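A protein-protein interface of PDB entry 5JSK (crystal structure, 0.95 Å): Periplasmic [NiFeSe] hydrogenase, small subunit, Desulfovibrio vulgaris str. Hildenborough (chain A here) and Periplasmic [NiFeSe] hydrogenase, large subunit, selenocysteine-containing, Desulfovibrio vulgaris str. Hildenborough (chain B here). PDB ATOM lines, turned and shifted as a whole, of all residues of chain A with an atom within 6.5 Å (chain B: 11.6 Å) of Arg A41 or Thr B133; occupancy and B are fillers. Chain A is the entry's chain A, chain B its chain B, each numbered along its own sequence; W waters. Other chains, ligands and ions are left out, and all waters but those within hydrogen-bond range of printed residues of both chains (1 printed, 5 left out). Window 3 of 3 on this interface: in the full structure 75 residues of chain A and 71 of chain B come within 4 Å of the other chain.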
ATOM      1  N   THR A  36      33.192 -18.392 -21.559  1.00  0.00           N
ATOM      2  CA  THR A  36      31.950 -17.747 -21.957  1.00  0.00           C
ATOM      3  C   THR A  36      30.805 -18.717 -21.726  1.00  0.00           C
ATOM      4  O   THR A  36      30.996 -19.937 -21.661  1.00  0.00           O
ATOM      5  CB  THR A  36      31.908 -17.352 -23.445  1.00  0.00           C
ATOM      6  OG1 THR A  36      32.235 -18.488 -24.262  1.00  0.00           O
ATOM      7  CG2 THR A  36      32.843 -16.209 -23.740  1.00  0.00           C
ATOM      8  N   LEU A  37      29.599 -18.155 -21.631  1.00  0.00           N
ATOM      9  CA  LEU A  37      28.405 -18.977 -21.491  1.00  0.00           C
ATOM     10  C   LEU A  37      28.219 -19.922 -22.672  1.00  0.00           C
ATOM     11  O   LEU A  37      27.537 -20.942 -22.531  1.00  0.00           O
ATOM     12  CB  LEU A  37      27.166 -18.084 -21.330  1.00  0.00           C
ATOM     13  CG  LEU A  37      27.137 -17.138 -20.123  1.00  0.00           C
ATOM     14  CD1 LEU A  37      25.858 -16.296 -20.109  1.00  0.00           C
ATOM     15  CD2 LEU A  37      27.261 -17.909 -18.821  1.00  0.00           C
ATOM     16  N   THR A  38      28.821 -19.618 -23.825  1.00  0.00           N
ATOM     17  CA  THR A  38      28.632 -20.404 -25.041  1.00  0.00           C
ATOM     18  C   THR A  38      29.904 -21.130 -25.480  1.00  0.00           C
ATOM     19  O   THR A  38      29.985 -21.596 -26.622  1.00  0.00           O
ATOM     20  CB  THR A  38      28.099 -19.514 -26.164  1.00  0.00           C
ATOM     21  OG1 THR A  38      29.013 -18.434 -26.390  1.00  0.00           O
ATOM     22  CG2 THR A  38      26.713 -18.964 -25.800  1.00  0.00           C
ATOM     23  N   GLY A  39      30.895 -21.252 -24.591  1.00  0.00           N
ATOM     24  CA  GLY A  39      32.128 -21.939 -24.916  1.00  0.00           C
ATOM     25  C   GLY A  39      32.040 -23.444 -24.692  1.00  0.00           C
ATOM     26  O   GLY A  39      31.022 -23.990 -24.263  1.00  0.00           O
ATOM     27  N   GLU A  40      33.144 -24.118 -25.003  1.00  0.00           N
ATOM     28  CA  GLU A  40      33.250 -25.555 -24.793  1.00  0.00           C
ATOM     29  C   GLU A  40      33.424 -25.841 -23.304  1.00  0.00           C
ATOM     30  O   GLU A  40      34.309 -25.272 -22.652  1.00  0.00           O
ATOM     31  CB  GLU A  40      34.453 -26.086 -25.573  1.00  0.00           C
ATOM     32  CG  GLU A  40      34.715 -27.588 -25.434  1.00  0.00           C
ATOM     33  CD  GLU A  40      35.795 -27.932 -24.414  1.00  0.00           C
ATOM     34  OE1 GLU A  40      36.642 -27.069 -24.103  1.00  0.00           O
ATOM     35  OE2 GLU A  40      35.801 -29.083 -23.931  1.00  0.00           O
ATOM     36  N   ARG A  41      32.562 -26.720 -22.759  1.00  0.00           N
ATOM     37  CA  ARG A  41      32.596 -27.092 -21.350  1.00  0.00           C
ATOM     38  C   ARG A  41      32.393 -28.594 -21.197  1.00  0.00           C
ATOM     39  O   ARG A  41      31.300 -29.096 -21.474  1.00  0.00           O
ATOM     40  CB  ARG A  41      31.499 -26.358 -20.585  1.00  0.00           C
ATOM     41  CG  ARG A  41      31.697 -24.862 -20.554  1.00  0.00           C
ATOM     42  CD  ARG A  41      30.606 -24.166 -19.776  1.00  0.00           C
ATOM     43  NE  ARG A  41      29.302 -24.309 -20.408  1.00  0.00           N
ATOM     44  CZ  ARG A  41      28.216 -24.819 -19.829  1.00  0.00           C
ATOM     45  NH1 ARG A  41      28.228 -25.235 -18.569  1.00  0.00           N
ATOM     46  NH2 ARG A  41      27.088 -24.898 -20.507  1.00  0.00           N
ATOM     47  N   PRO A  42      33.401 -29.340 -20.745  1.00  0.00           N
ATOM     48  CA  PRO A  42      33.274 -30.795 -20.712  1.00  0.00           C
ATOM     49  C   PRO A  42      32.331 -31.251 -19.617  1.00  0.00           C
ATOM     50  O   PRO A  42      32.189 -30.586 -18.575  1.00  0.00           O
ATOM     51  CB  PRO A  42      34.709 -31.269 -20.430  1.00  0.00           C
ATOM     52  CG  PRO A  42      35.296 -30.147 -19.699  1.00  0.00           C
ATOM     53  CD  PRO A  42      34.737 -28.909 -20.328  1.00  0.00           C
ATOM     54  N   PRO A  43      31.708 -32.416 -19.786  1.00  0.00           N
ATOM     55  CA  PRO A  43      30.795 -32.938 -18.768  1.00  0.00           C
ATOM     56  C   PRO A  43      31.537 -33.530 -17.584  1.00  0.00           C
ATOM     57  O   PRO A  43      32.554 -34.214 -17.729  1.00  0.00           O
ATOM     58  CB  PRO A  43      30.029 -34.028 -19.526  1.00  0.00           C
ATOM     59  CG  PRO A  43      30.975 -34.467 -20.600  1.00  0.00           C
ATOM     60  CD  PRO A  43      31.761 -33.274 -20.983  1.00  0.00           C
ATOM     61  N   ASP A  69      31.105 -18.820 -12.201  1.00  0.00           N
ATOM     62  CA  ASP A  69      31.838 -18.859 -13.458  1.00  0.00           C
ATOM     63  C   ASP A  69      32.326 -20.268 -13.787  1.00  0.00           C
ATOM     64  O   ASP A  69      32.312 -20.671 -14.956  1.00  0.00           O
ATOM     65  CB  ASP A  69      32.969 -17.829 -13.449  1.00  0.00           C
ATOM     66  CG  ASP A  69      32.460 -16.376 -13.674  1.00  0.00           C
ATOM     67  OD1 ASP A  69      31.323 -16.193 -14.175  1.00  0.00           O
ATOM     68  OD2 ASP A  69      33.208 -15.421 -13.383  1.00  0.00           O
ATOM     69  N   VAL A  70      32.753 -21.037 -12.784  1.00  0.00           N
ATOM     70  CA  VAL A  70      33.143 -22.418 -13.047  1.00  0.00           C
ATOM     71  C   VAL A  70      31.977 -23.185 -13.664  1.00  0.00           C
ATOM     72  O   VAL A  70      32.129 -23.883 -14.676  1.00  0.00           O
ATOM     73  CB  VAL A  70      33.646 -23.090 -11.759  1.00  0.00           C
ATOM     74  CG1 VAL A  70      33.845 -24.576 -11.972  1.00  0.00           C
ATOM     75  CG2 VAL A  70      34.945 -22.435 -11.307  1.00  0.00           C
ATOM     76  N   LEU A  71      30.792 -23.074 -13.053  1.00  0.00           N
ATOM     77  CA  LEU A  71      29.644 -23.860 -13.498  1.00  0.00           C
ATOM     78  C   LEU A  71      29.103 -23.403 -14.840  1.00  0.00           C
ATOM     79  O   LEU A  71      28.580 -24.227 -15.600  1.00  0.00           O
ATOM     80  CB  LEU A  71      28.519 -23.791 -12.469  1.00  0.00           C
ATOM     81  CG  LEU A  71      28.823 -24.392 -11.103  1.00  0.00           C
ATOM     82  CD1 LEU A  71      27.613 -24.259 -10.198  1.00  0.00           C
ATOM     83  CD2 LEU A  71      29.232 -25.848 -11.235  1.00  0.00           C
ATOM     84  N   LEU A  72      29.173 -22.106 -15.132  1.00  0.00           N
ATOM     85  CA  LEU A  72      28.518 -21.594 -16.323  1.00  0.00           C
ATOM     86  C   LEU A  72      29.470 -21.423 -17.486  1.00  0.00           C
ATOM     87  O   LEU A  72      29.009 -21.318 -18.629  1.00  0.00           O
ATOM     88  CB  LEU A  72      27.802 -20.269 -16.016  1.00  0.00           C
ATOM     89  CG  LEU A  72      26.649 -20.374 -15.007  1.00  0.00           C
ATOM     90  CD1 LEU A  72      26.119 -18.995 -14.657  1.00  0.00           C
ATOM     91  CD2 LEU A  72      25.530 -21.242 -15.552  1.00  0.00           C
ATOM     92  N   LYS A  73      30.786 -21.399 -17.224  1.00  0.00           N
ATOM     93  CA  LYS A  73      31.774 -21.073 -18.239  1.00  0.00           C
ATOM     94  C   LYS A  73      32.924 -22.065 -18.379  1.00  0.00           C
ATOM     95  O   LYS A  73      33.642 -21.977 -19.381  1.00  0.00           O
ATOM     96  CB  LYS A  73      32.375 -19.677 -17.978  1.00  0.00           C
ATOM     97  CG  LYS A  73      31.356 -18.553 -17.939  1.00  0.00           C
ATOM     98  CD  LYS A  73      32.013 -17.213 -17.655  1.00  0.00           C
ATOM     99  CE  LYS A  73      30.989 -16.093 -17.572  1.00  0.00           C
ATOM    100  NZ  LYS A  73      31.610 -14.793 -17.179  1.00  0.00           N
ATOM    101  N   VAL A  74      33.145 -22.982 -17.418  1.00  0.00           N
ATOM    102  CA  VAL A  74      34.326 -23.849 -17.427  1.00  0.00           C
ATOM    103  C   VAL A  74      33.959 -25.322 -17.600  1.00  0.00           C
ATOM    104  O   VAL A  74      34.527 -26.014 -18.451  1.00  0.00           O
ATOM    105  CB  VAL A  74      35.197 -23.641 -16.168  1.00  0.00           C
ATOM    106  CG1 VAL A  74      36.429 -24.548 -16.227  1.00  0.00           C
ATOM    107  CG2 VAL A  74      35.621 -22.180 -16.022  1.00  0.00           C
ATOM    108  N   ILE A  75      33.050 -25.836 -16.771  1.00  0.00           N
ATOM    109  CA  ILE A  75      32.623 -27.230 -16.837  1.00  0.00           C
ATOM    110  C   ILE A  75      31.114 -27.268 -17.011  1.00  0.00           C
ATOM    111  O   ILE A  75      30.417 -26.275 -16.794  1.00  0.00           O
ATOM    112  CB  ILE A  75      33.036 -28.049 -15.592  1.00  0.00           C
ATOM    113  CG1 ILE A  75      32.319 -27.535 -14.332  1.00  0.00           C
ATOM    114  CG2 ILE A  75      34.537 -28.027 -15.417  1.00  0.00           C
ATOM    115  CD1 ILE A  75      32.553 -28.369 -13.086  1.00  0.00           C
ATOM    116  N   SER A  76      30.614 -28.449 -17.379  1.00  0.00           N
ATOM    117  CA  SER A  76      29.181 -28.740 -17.357  1.00  0.00           C
ATOM    118  C   SER A  76      28.945 -29.797 -16.288  1.00  0.00           C
ATOM    119  O   SER A  76      29.188 -30.987 -16.514  1.00  0.00           O
ATOM    120  CB  SER A  76      28.689 -29.227 -18.710  1.00  0.00           C
ATOM    121  OG  SER A  76      27.285 -29.297 -18.700  1.00  0.00           O
ATOM    122  N   LEU A  77      28.483 -29.352 -15.120  1.00  0.00           N
ATOM    123  CA  LEU A  77      28.281 -30.235 -13.976  1.00  0.00           C
ATOM    124  C   LEU A  77      26.930 -30.923 -14.141  1.00  0.00           C
ATOM    125  O   LEU A  77      25.884 -30.365 -13.800  1.00  0.00           O
ATOM    126  CB  LEU A  77      28.365 -29.438 -12.685  1.00  0.00           C
ATOM    127  CG  LEU A  77      28.256 -30.267 -11.401  1.00  0.00           C
ATOM    128  CD1 LEU A  77      29.387 -31.289 -11.279  1.00  0.00           C
ATOM    129  CD2 LEU A  77      28.225 -29.323 -10.213  1.00  0.00           C
ATOM    130  N   GLU A  78      26.963 -32.132 -14.700  1.00  0.00           N
ATOM    131  CA  GLU A  78      25.753 -32.813 -15.137  1.00  0.00           C
ATOM    132  C   GLU A  78      25.066 -33.588 -14.022  1.00  0.00           C
ATOM    133  O   GLU A  78      23.844 -33.767 -14.069  1.00  0.00           O
ATOM    134  CB  GLU A  78      26.099 -33.745 -16.294  1.00  0.00           C
ATOM    135  CG  GLU A  78      26.531 -33.009 -17.561  1.00  0.00           C
ATOM    136  CD  GLU A  78      25.410 -32.260 -18.253  1.00  0.00           C
ATOM    137  OE1 GLU A  78      24.223 -32.519 -17.957  1.00  0.00           O
ATOM    138  OE2 GLU A  78      25.724 -31.389 -19.103  1.00  0.00           O
ATOM    139  N   PHE A 102      29.072 -39.430 -23.995  1.00  0.00           N
ATOM    140  CA  PHE A 102      30.430 -38.954 -23.780  1.00  0.00           C
ATOM    141  C   PHE A 102      31.331 -40.059 -23.248  1.00  0.00           C
ATOM    142  O   PHE A 102      32.245 -39.811 -22.459  1.00  0.00           O
ATOM    143  CB  PHE A 102      30.443 -37.744 -22.848  1.00  0.00           C
ATOM    144  CG  PHE A 102      29.908 -36.500 -23.467  1.00  0.00           C
ATOM    145  CD1 PHE A 102      30.728 -35.679 -24.216  1.00  0.00           C
ATOM    146  CD2 PHE A 102      28.583 -36.139 -23.294  1.00  0.00           C
ATOM    147  CE1 PHE A 102      30.241 -34.524 -24.786  1.00  0.00           C
ATOM    148  CE2 PHE A 102      28.086 -34.989 -23.864  1.00  0.00           C
ATOM    149  CZ  PHE A 102      28.916 -34.177 -24.612  1.00  0.00           C
ATOM    150  N   ARG B  23      19.689 -32.030  -3.498  1.00  0.00           N
ATOM    151  CA  ARG B  23      19.540 -30.710  -2.905  1.00  0.00           C
ATOM    152  C   ARG B  23      19.205 -30.807  -1.419  1.00  0.00           C
ATOM    153  O   ARG B  23      18.378 -30.076  -0.867  1.00  0.00           O
ATOM    154  CB  ARG B  23      18.628 -29.799  -3.719  1.00  0.00           C
ATOM    155  CG  ARG B  23      19.375 -29.243  -4.927  1.00  0.00           C
ATOM    156  CD  ARG B  23      18.512 -28.356  -5.799  1.00  0.00           C
ATOM    157  NE  ARG B  23      17.396 -29.064  -6.421  1.00  0.00           N
ATOM    158  CZ  ARG B  23      16.111 -28.928  -6.089  1.00  0.00           C
ATOM    159  NH1 ARG B  23      15.727 -28.127  -5.097  1.00  0.00           N
ATOM    160  NH2 ARG B  23      15.195 -29.602  -6.764  1.00  0.00           N
ATOM    161  N   GLN B 125      15.483 -23.898  -6.064  1.00  0.00           N
ATOM    162  CA  GLN B 125      15.085 -24.540  -7.308  1.00  0.00           C
ATOM    163  C   GLN B 125      13.762 -25.287  -7.182  1.00  0.00           C
ATOM    164  O   GLN B 125      13.170 -25.626  -8.212  1.00  0.00           O
ATOM    165  CB  GLN B 125      16.172 -25.457  -7.861  1.00  0.00           C
ATOM    166  CG  GLN B 125      17.339 -24.717  -8.481  1.00  0.00           C
ATOM    167  CD  GLN B 125      18.233 -25.652  -9.256  1.00  0.00           C
ATOM    168  OE1 GLN B 125      17.897 -26.055 -10.362  1.00  0.00           O
ATOM    169  NE2 GLN B 125      19.367 -26.035  -8.666  1.00  0.00           N
ATOM    170  N   VAL B 128      11.927 -22.027  -8.332  1.00  0.00           N
ATOM    171  CA  VAL B 128      12.585 -21.158  -9.303  1.00  0.00           C
ATOM    172  C   VAL B 128      13.188 -22.028 -10.403  1.00  0.00           C
ATOM    173  O   VAL B 128      13.927 -22.978 -10.122  1.00  0.00           O
ATOM    174  CB  VAL B 128      13.689 -20.321  -8.623  1.00  0.00           C
ATOM    175  CG1 VAL B 128      14.418 -19.469  -9.647  1.00  0.00           C
ATOM    176  CG2 VAL B 128      13.127 -19.468  -7.503  1.00  0.00           C
ATOM    177  N   GLN B 129      12.904 -21.675 -11.656  1.00  0.00           N
ATOM    178  CA  GLN B 129      13.533 -22.312 -12.808  1.00  0.00           C
ATOM    179  C   GLN B 129      14.893 -21.673 -13.063  1.00  0.00           C
ATOM    180  O   GLN B 129      14.976 -20.464 -13.304  1.00  0.00           O
ATOM    181  CB  GLN B 129      12.664 -22.114 -14.051  1.00  0.00           C
ATOM    182  CG  GLN B 129      13.335 -22.581 -15.351  1.00  0.00           C
ATOM    183  CD  GLN B 129      13.579 -24.080 -15.383  1.00  0.00           C
ATOM    184  OE1 GLN B 129      12.642 -24.866 -15.321  1.00  0.00           O
ATOM    185  NE2 GLN B 129      14.842 -24.477 -15.454  1.00  0.00           N
ATOM    186  N   GLY B 130      15.955 -22.478 -13.035  1.00  0.00           N
ATOM    187  CA  GLY B 130      17.275 -21.977 -13.334  1.00  0.00           C
ATOM    188  C   GLY B 130      17.534 -21.907 -14.824  1.00  0.00           C
ATOM    189  O   GLY B 130      16.705 -22.301 -15.648  1.00  0.00           O
ATOM    190  N   PRO B 131      18.720 -21.406 -15.186  1.00  0.00           N
ATOM    191  CA  PRO B 131      19.083 -21.306 -16.604  1.00  0.00           C
ATOM    192  C   PRO B 131      19.153 -22.670 -17.282  1.00  0.00           C
ATOM    193  O   PRO B 131      19.232 -23.722 -16.643  1.00  0.00           O
ATOM    194  CB  PRO B 131      20.454 -20.621 -16.579  1.00  0.00           C
ATOM    195  CG  PRO B 131      20.960 -20.761 -15.219  1.00  0.00           C
ATOM    196  CD  PRO B 131      19.788 -20.915 -14.299  1.00  0.00           C
ATOM    197  N   ASP B 132      19.115 -22.636 -18.614  1.00  0.00           N
ATOM    198  CA  ASP B 132      18.961 -23.847 -19.419  1.00  0.00           C
ATOM    199  C   ASP B 132      20.306 -24.542 -19.650  1.00  0.00           C
ATOM    200  O   ASP B 132      20.753 -24.742 -20.774  1.00  0.00           O
ATOM    201  CB  ASP B 132      18.286 -23.496 -20.737  1.00  0.00           C
ATOM    202  CG  ASP B 132      17.950 -24.713 -21.561  1.00  0.00           C
ATOM    203  OD1 ASP B 132      17.691 -25.785 -20.984  1.00  0.00           O
ATOM    204  OD2 ASP B 132      17.930 -24.590 -22.807  1.00  0.00           O
ATOM    205  N   THR B 133      20.947 -24.929 -18.552  1.00  0.00           N
ATOM    206  CA  THR B 133      22.152 -25.733 -18.636  1.00  0.00           C
ATOM    207  C   THR B 133      22.340 -26.444 -17.301  1.00  0.00           C
ATOM    208  O   THR B 133      21.805 -26.021 -16.268  1.00  0.00           O
ATOM    209  CB  THR B 133      23.339 -24.858 -19.024  1.00  0.00           C
ATOM    210  OG1 THR B 133      24.370 -25.681 -19.591  1.00  0.00           O
ATOM    211  CG2 THR B 133      23.843 -24.050 -17.817  1.00  0.00           C
ATOM    212  N   ALA B 134      23.052 -27.568 -17.337  1.00  0.00           N
ATOM    213  CA  ALA B 134      23.304 -28.315 -16.107  1.00  0.00           C
ATOM    214  C   ALA B 134      24.075 -27.431 -15.114  1.00  0.00           C
ATOM    215  O   ALA B 134      24.926 -26.655 -15.519  1.00  0.00           O
ATOM    216  CB  ALA B 134      24.078 -29.593 -16.403  1.00  0.00           C
ATOM    217  N   PRO B 135      23.812 -27.563 -13.806  1.00  0.00           N
ATOM    218  CA  PRO B 135      22.989 -28.576 -13.155  1.00  0.00           C
ATOM    219  C   PRO B 135      21.539 -28.160 -12.923  1.00  0.00           C
ATOM    220  O   PRO B 135      20.885 -28.729 -12.062  1.00  0.00           O
ATOM    221  CB  PRO B 135      23.719 -28.751 -11.822  1.00  0.00           C
ATOM    222  CG  PRO B 135      24.174 -27.363 -11.516  1.00  0.00           C
ATOM    223  CD  PRO B 135      24.611 -26.801 -12.828  1.00  0.00           C
ATOM    224  N   PHE B 136      21.036 -27.192 -13.689  1.00  0.00           N
ATOM    225  CA  PHE B 136      19.693 -26.652 -13.502  1.00  0.00           C
ATOM    226  C   PHE B 136      18.639 -27.329 -14.368  1.00  0.00           C
ATOM    227  O   PHE B 136      17.437 -27.080 -14.179  1.00  0.00           O
ATOM    228  CB  PHE B 136      19.708 -25.152 -13.787  1.00  0.00           C
ATOM    229  CG  PHE B 136      20.729 -24.420 -12.977  1.00  0.00           C
ATOM    230  CD1 PHE B 136      20.507 -24.199 -11.632  1.00  0.00           C
ATOM    231  CD2 PHE B 136      21.924 -23.989 -13.528  1.00  0.00           C
ATOM    232  CE1 PHE B 136      21.441 -23.550 -10.863  1.00  0.00           C
ATOM    233  CE2 PHE B 136      22.865 -23.330 -12.753  1.00  0.00           C
ATOM    234  CZ  PHE B 136      22.618 -23.117 -11.423  1.00  0.00           C
ATOM    235  N   VAL B 137      19.076 -28.144 -15.316  1.00  0.00           N
ATOM    236  CA  VAL B 137      18.251 -28.963 -16.196  1.00  0.00           C
ATOM    237  C   VAL B 137      19.036 -30.257 -16.412  1.00  0.00           C
ATOM    238  O   VAL B 137      20.261 -30.274 -16.252  1.00  0.00           O
ATOM    239  CB  VAL B 137      17.965 -28.275 -17.549  1.00  0.00           C
ATOM    240  CG1 VAL B 137      17.142 -27.012 -17.376  1.00  0.00           C
ATOM    241  CG2 VAL B 137      19.261 -27.993 -18.302  1.00  0.00           C
ATOM    242  N   PRO B 138      18.368 -31.340 -16.810  1.00  0.00           N
ATOM    243  CA  PRO B 138      16.916 -31.481 -16.910  1.00  0.00           C
ATOM    244  C   PRO B 138      16.269 -31.596 -15.526  1.00  0.00           C
ATOM    245  O   PRO B 138      16.953 -31.777 -14.509  1.00  0.00           O
ATOM    246  CB  PRO B 138      16.757 -32.787 -17.695  1.00  0.00           C
ATOM    247  CG  PRO B 138      17.945 -33.595 -17.291  1.00  0.00           C
ATOM    248  CD  PRO B 138      19.070 -32.603 -17.093  1.00  0.00           C
ATOM    249  N   ARG B 139      14.949 -31.491 -15.487  1.00  0.00           N
ATOM    250  CA  ARG B 139      14.188 -31.634 -14.249  1.00  0.00           C
ATOM    251  C   ARG B 139      12.790 -32.130 -14.614  1.00  0.00           C
ATOM    252  O   ARG B 139      12.512 -32.453 -15.770  1.00  0.00           O
ATOM    253  CB  ARG B 139      14.219 -30.337 -13.430  1.00  0.00           C
ATOM    254  CG  ARG B 139      13.605 -29.140 -14.133  1.00  0.00           C
ATOM    255  CD  ARG B 139      13.715 -27.875 -13.307  1.00  0.00           C
ATOM    256  NE  ARG B 139      12.943 -28.032 -12.094  1.00  0.00           N
ATOM    257  CZ  ARG B 139      12.997 -27.230 -11.042  1.00  0.00           C
ATOM    258  NH1 ARG B 139      13.780 -26.169 -11.040  1.00  0.00           N
ATOM    259  NH2 ARG B 139      12.235 -27.481  -9.996  1.00  0.00           N
ATOM    260  N   VAL B 156      16.743 -16.141  -9.457  1.00  0.00           N
ATOM    261  CA  VAL B 156      18.009 -16.523 -10.077  1.00  0.00           C
ATOM    262  C   VAL B 156      19.104 -15.524  -9.714  1.00  0.00           C
ATOM    263  O   VAL B 156      20.224 -15.898  -9.342  1.00  0.00           O
ATOM    264  CB  VAL B 156      17.851 -16.662 -11.602  1.00  0.00           C
ATOM    265  CG1 VAL B 156      19.212 -16.879 -12.248  1.00  0.00           C
ATOM    266  CG2 VAL B 156      16.903 -17.800 -11.946  1.00  0.00           C
ATOM    267  N   TYR B 159      20.079 -16.097  -6.164  1.00  0.00           N
ATOM    268  CA  TYR B 159      20.883 -17.317  -6.059  1.00  0.00           C
ATOM    269  C   TYR B 159      22.343 -17.011  -6.377  1.00  0.00           C
ATOM    270  O   TYR B 159      23.261 -17.429  -5.661  1.00  0.00           O
ATOM    271  CB  TYR B 159      20.309 -18.368  -7.020  1.00  0.00           C
ATOM    272  CG  TYR B 159      21.029 -19.701  -7.147  1.00  0.00           C
ATOM    273  CD1 TYR B 159      22.260 -19.814  -7.782  1.00  0.00           C
ATOM    274  CD2 TYR B 159      20.428 -20.868  -6.717  1.00  0.00           C
ATOM    275  CE1 TYR B 159      22.875 -21.049  -7.948  1.00  0.00           C
ATOM    276  CE2 TYR B 159      21.024 -22.109  -6.893  1.00  0.00           C
ATOM    277  CZ  TYR B 159      22.263 -22.190  -7.500  1.00  0.00           C
ATOM    278  OH  TYR B 159      22.912 -23.383  -7.699  1.00  0.00           O
ATOM    279  N   ILE B 160      22.566 -16.288  -7.477  1.00  0.00           N
ATOM    280  CA  ILE B 160      23.918 -15.956  -7.908  1.00  0.00           C
ATOM    281  C   ILE B 160      24.600 -15.045  -6.893  1.00  0.00           C
ATOM    282  O   ILE B 160      25.753 -15.271  -6.514  1.00  0.00           O
ATOM    283  CB  ILE B 160      23.875 -15.346  -9.318  1.00  0.00           C
ATOM    284  CG1 ILE B 160      23.439 -16.408 -10.329  1.00  0.00           C
ATOM    285  CG2 ILE B 160      25.226 -14.780  -9.698  1.00  0.00           C
ATOM    286  CD1 ILE B 160      23.083 -15.838 -11.666  1.00  0.00           C
HETATM  287  O   HOH W   1      21.760 -31.663 -14.178  1.00  0.00           O
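CG2 of Thr B133 touches CD2 of Leu A72, 3.98 Å away.
OG of Ser A76 touches CB of Ala B134, at 3.96 Å.
O of Leu A77 touches CB of Ala B134, at 3.3 Å.
CB of Ala B134 touches OE1 of Glu A78 (3.3 Å).
The guanidinium group of Arg A41 lies within hydrogen-bond range of the backbone carbonyl oxygen of Leu A71 (3.2 Å).
The guanidinium group (NE) of Arg A41 sits close to the backbone carbonyl oxygen (O) of Leu A72.
O of Ile A75 is in hydrogen-bond range of NH1 of Arg A41, at 3.0 Å.
The backbone NH (N) of Ser A76 sits at hydrogen-bond distance from the backbone carbonyl oxygen (O) of Pro A42, at 2.9 Å.
The side-chain hydroxyl of Ser A76 lies within hydrogen-bond range of the side-chain carboxylate of Glu A78, 2.6 Å away.
Printed residues of chain A within 4 Å of Thr B133: Arg A41 (3.0 Å) and Leu A72 (3.98 Å).
No residue of chain B comes within 4 Å of Gly A39.
No residue of chain B comes within 4 Å of Glu A40.
No residue of chain B comes within 4 Å of Pro A42.
No residue of chain B comes within 4 Å of Pro A43.
No residue of chain B comes within 4 Å of Val A74.
Ser A76 touches one residue of chain B.
Of the printed residues of chain A, Ala B134 touches Ser A76, Leu A77 and Glu A78.
Of the printed residues of chain B, Leu A72 touches Thr B133 (3.98 Å).
Phe A102 touches none of the printed residues of chain B.
The nearest residue of chain B that does not touch Arg A41 is Ala B134 (4.7 Å).
The nearest printed residue of chain B that does not touch Glu A78 is Val B137 (4.9 Å).
Water W1 bridges the backbone carbonyl oxygen (O) of Val B137 (2.9 Å) and the backbone carbonyl oxygen (O) of Glu A78 (3.0 Å).
Of the 17 printed residues of chain B, 3 touch a printed residue of chain A.
Hydrophobic or aromatic side chains of chain B that line the printed part of chain A: Ala B134 and Pro B135.
Hydrophobic or aromatic side chains of chain A that line the printed part of chain B: Leu A72.
Among the printed residues, no Asp or Glu carboxylate lies within 4 Å of a Lys or Arg side-chain nitrogen of the other chain.
The guanidinium group (NH2) of Arg A41 lies within hydrogen-bond range of the side-chain hydroxyl (OG1) of Thr B133 (3.0 Å).
The backbone carbonyl oxygen of Leu A77 lies close to the backbone nitrogen of Pro B135, 3.5 Å away.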
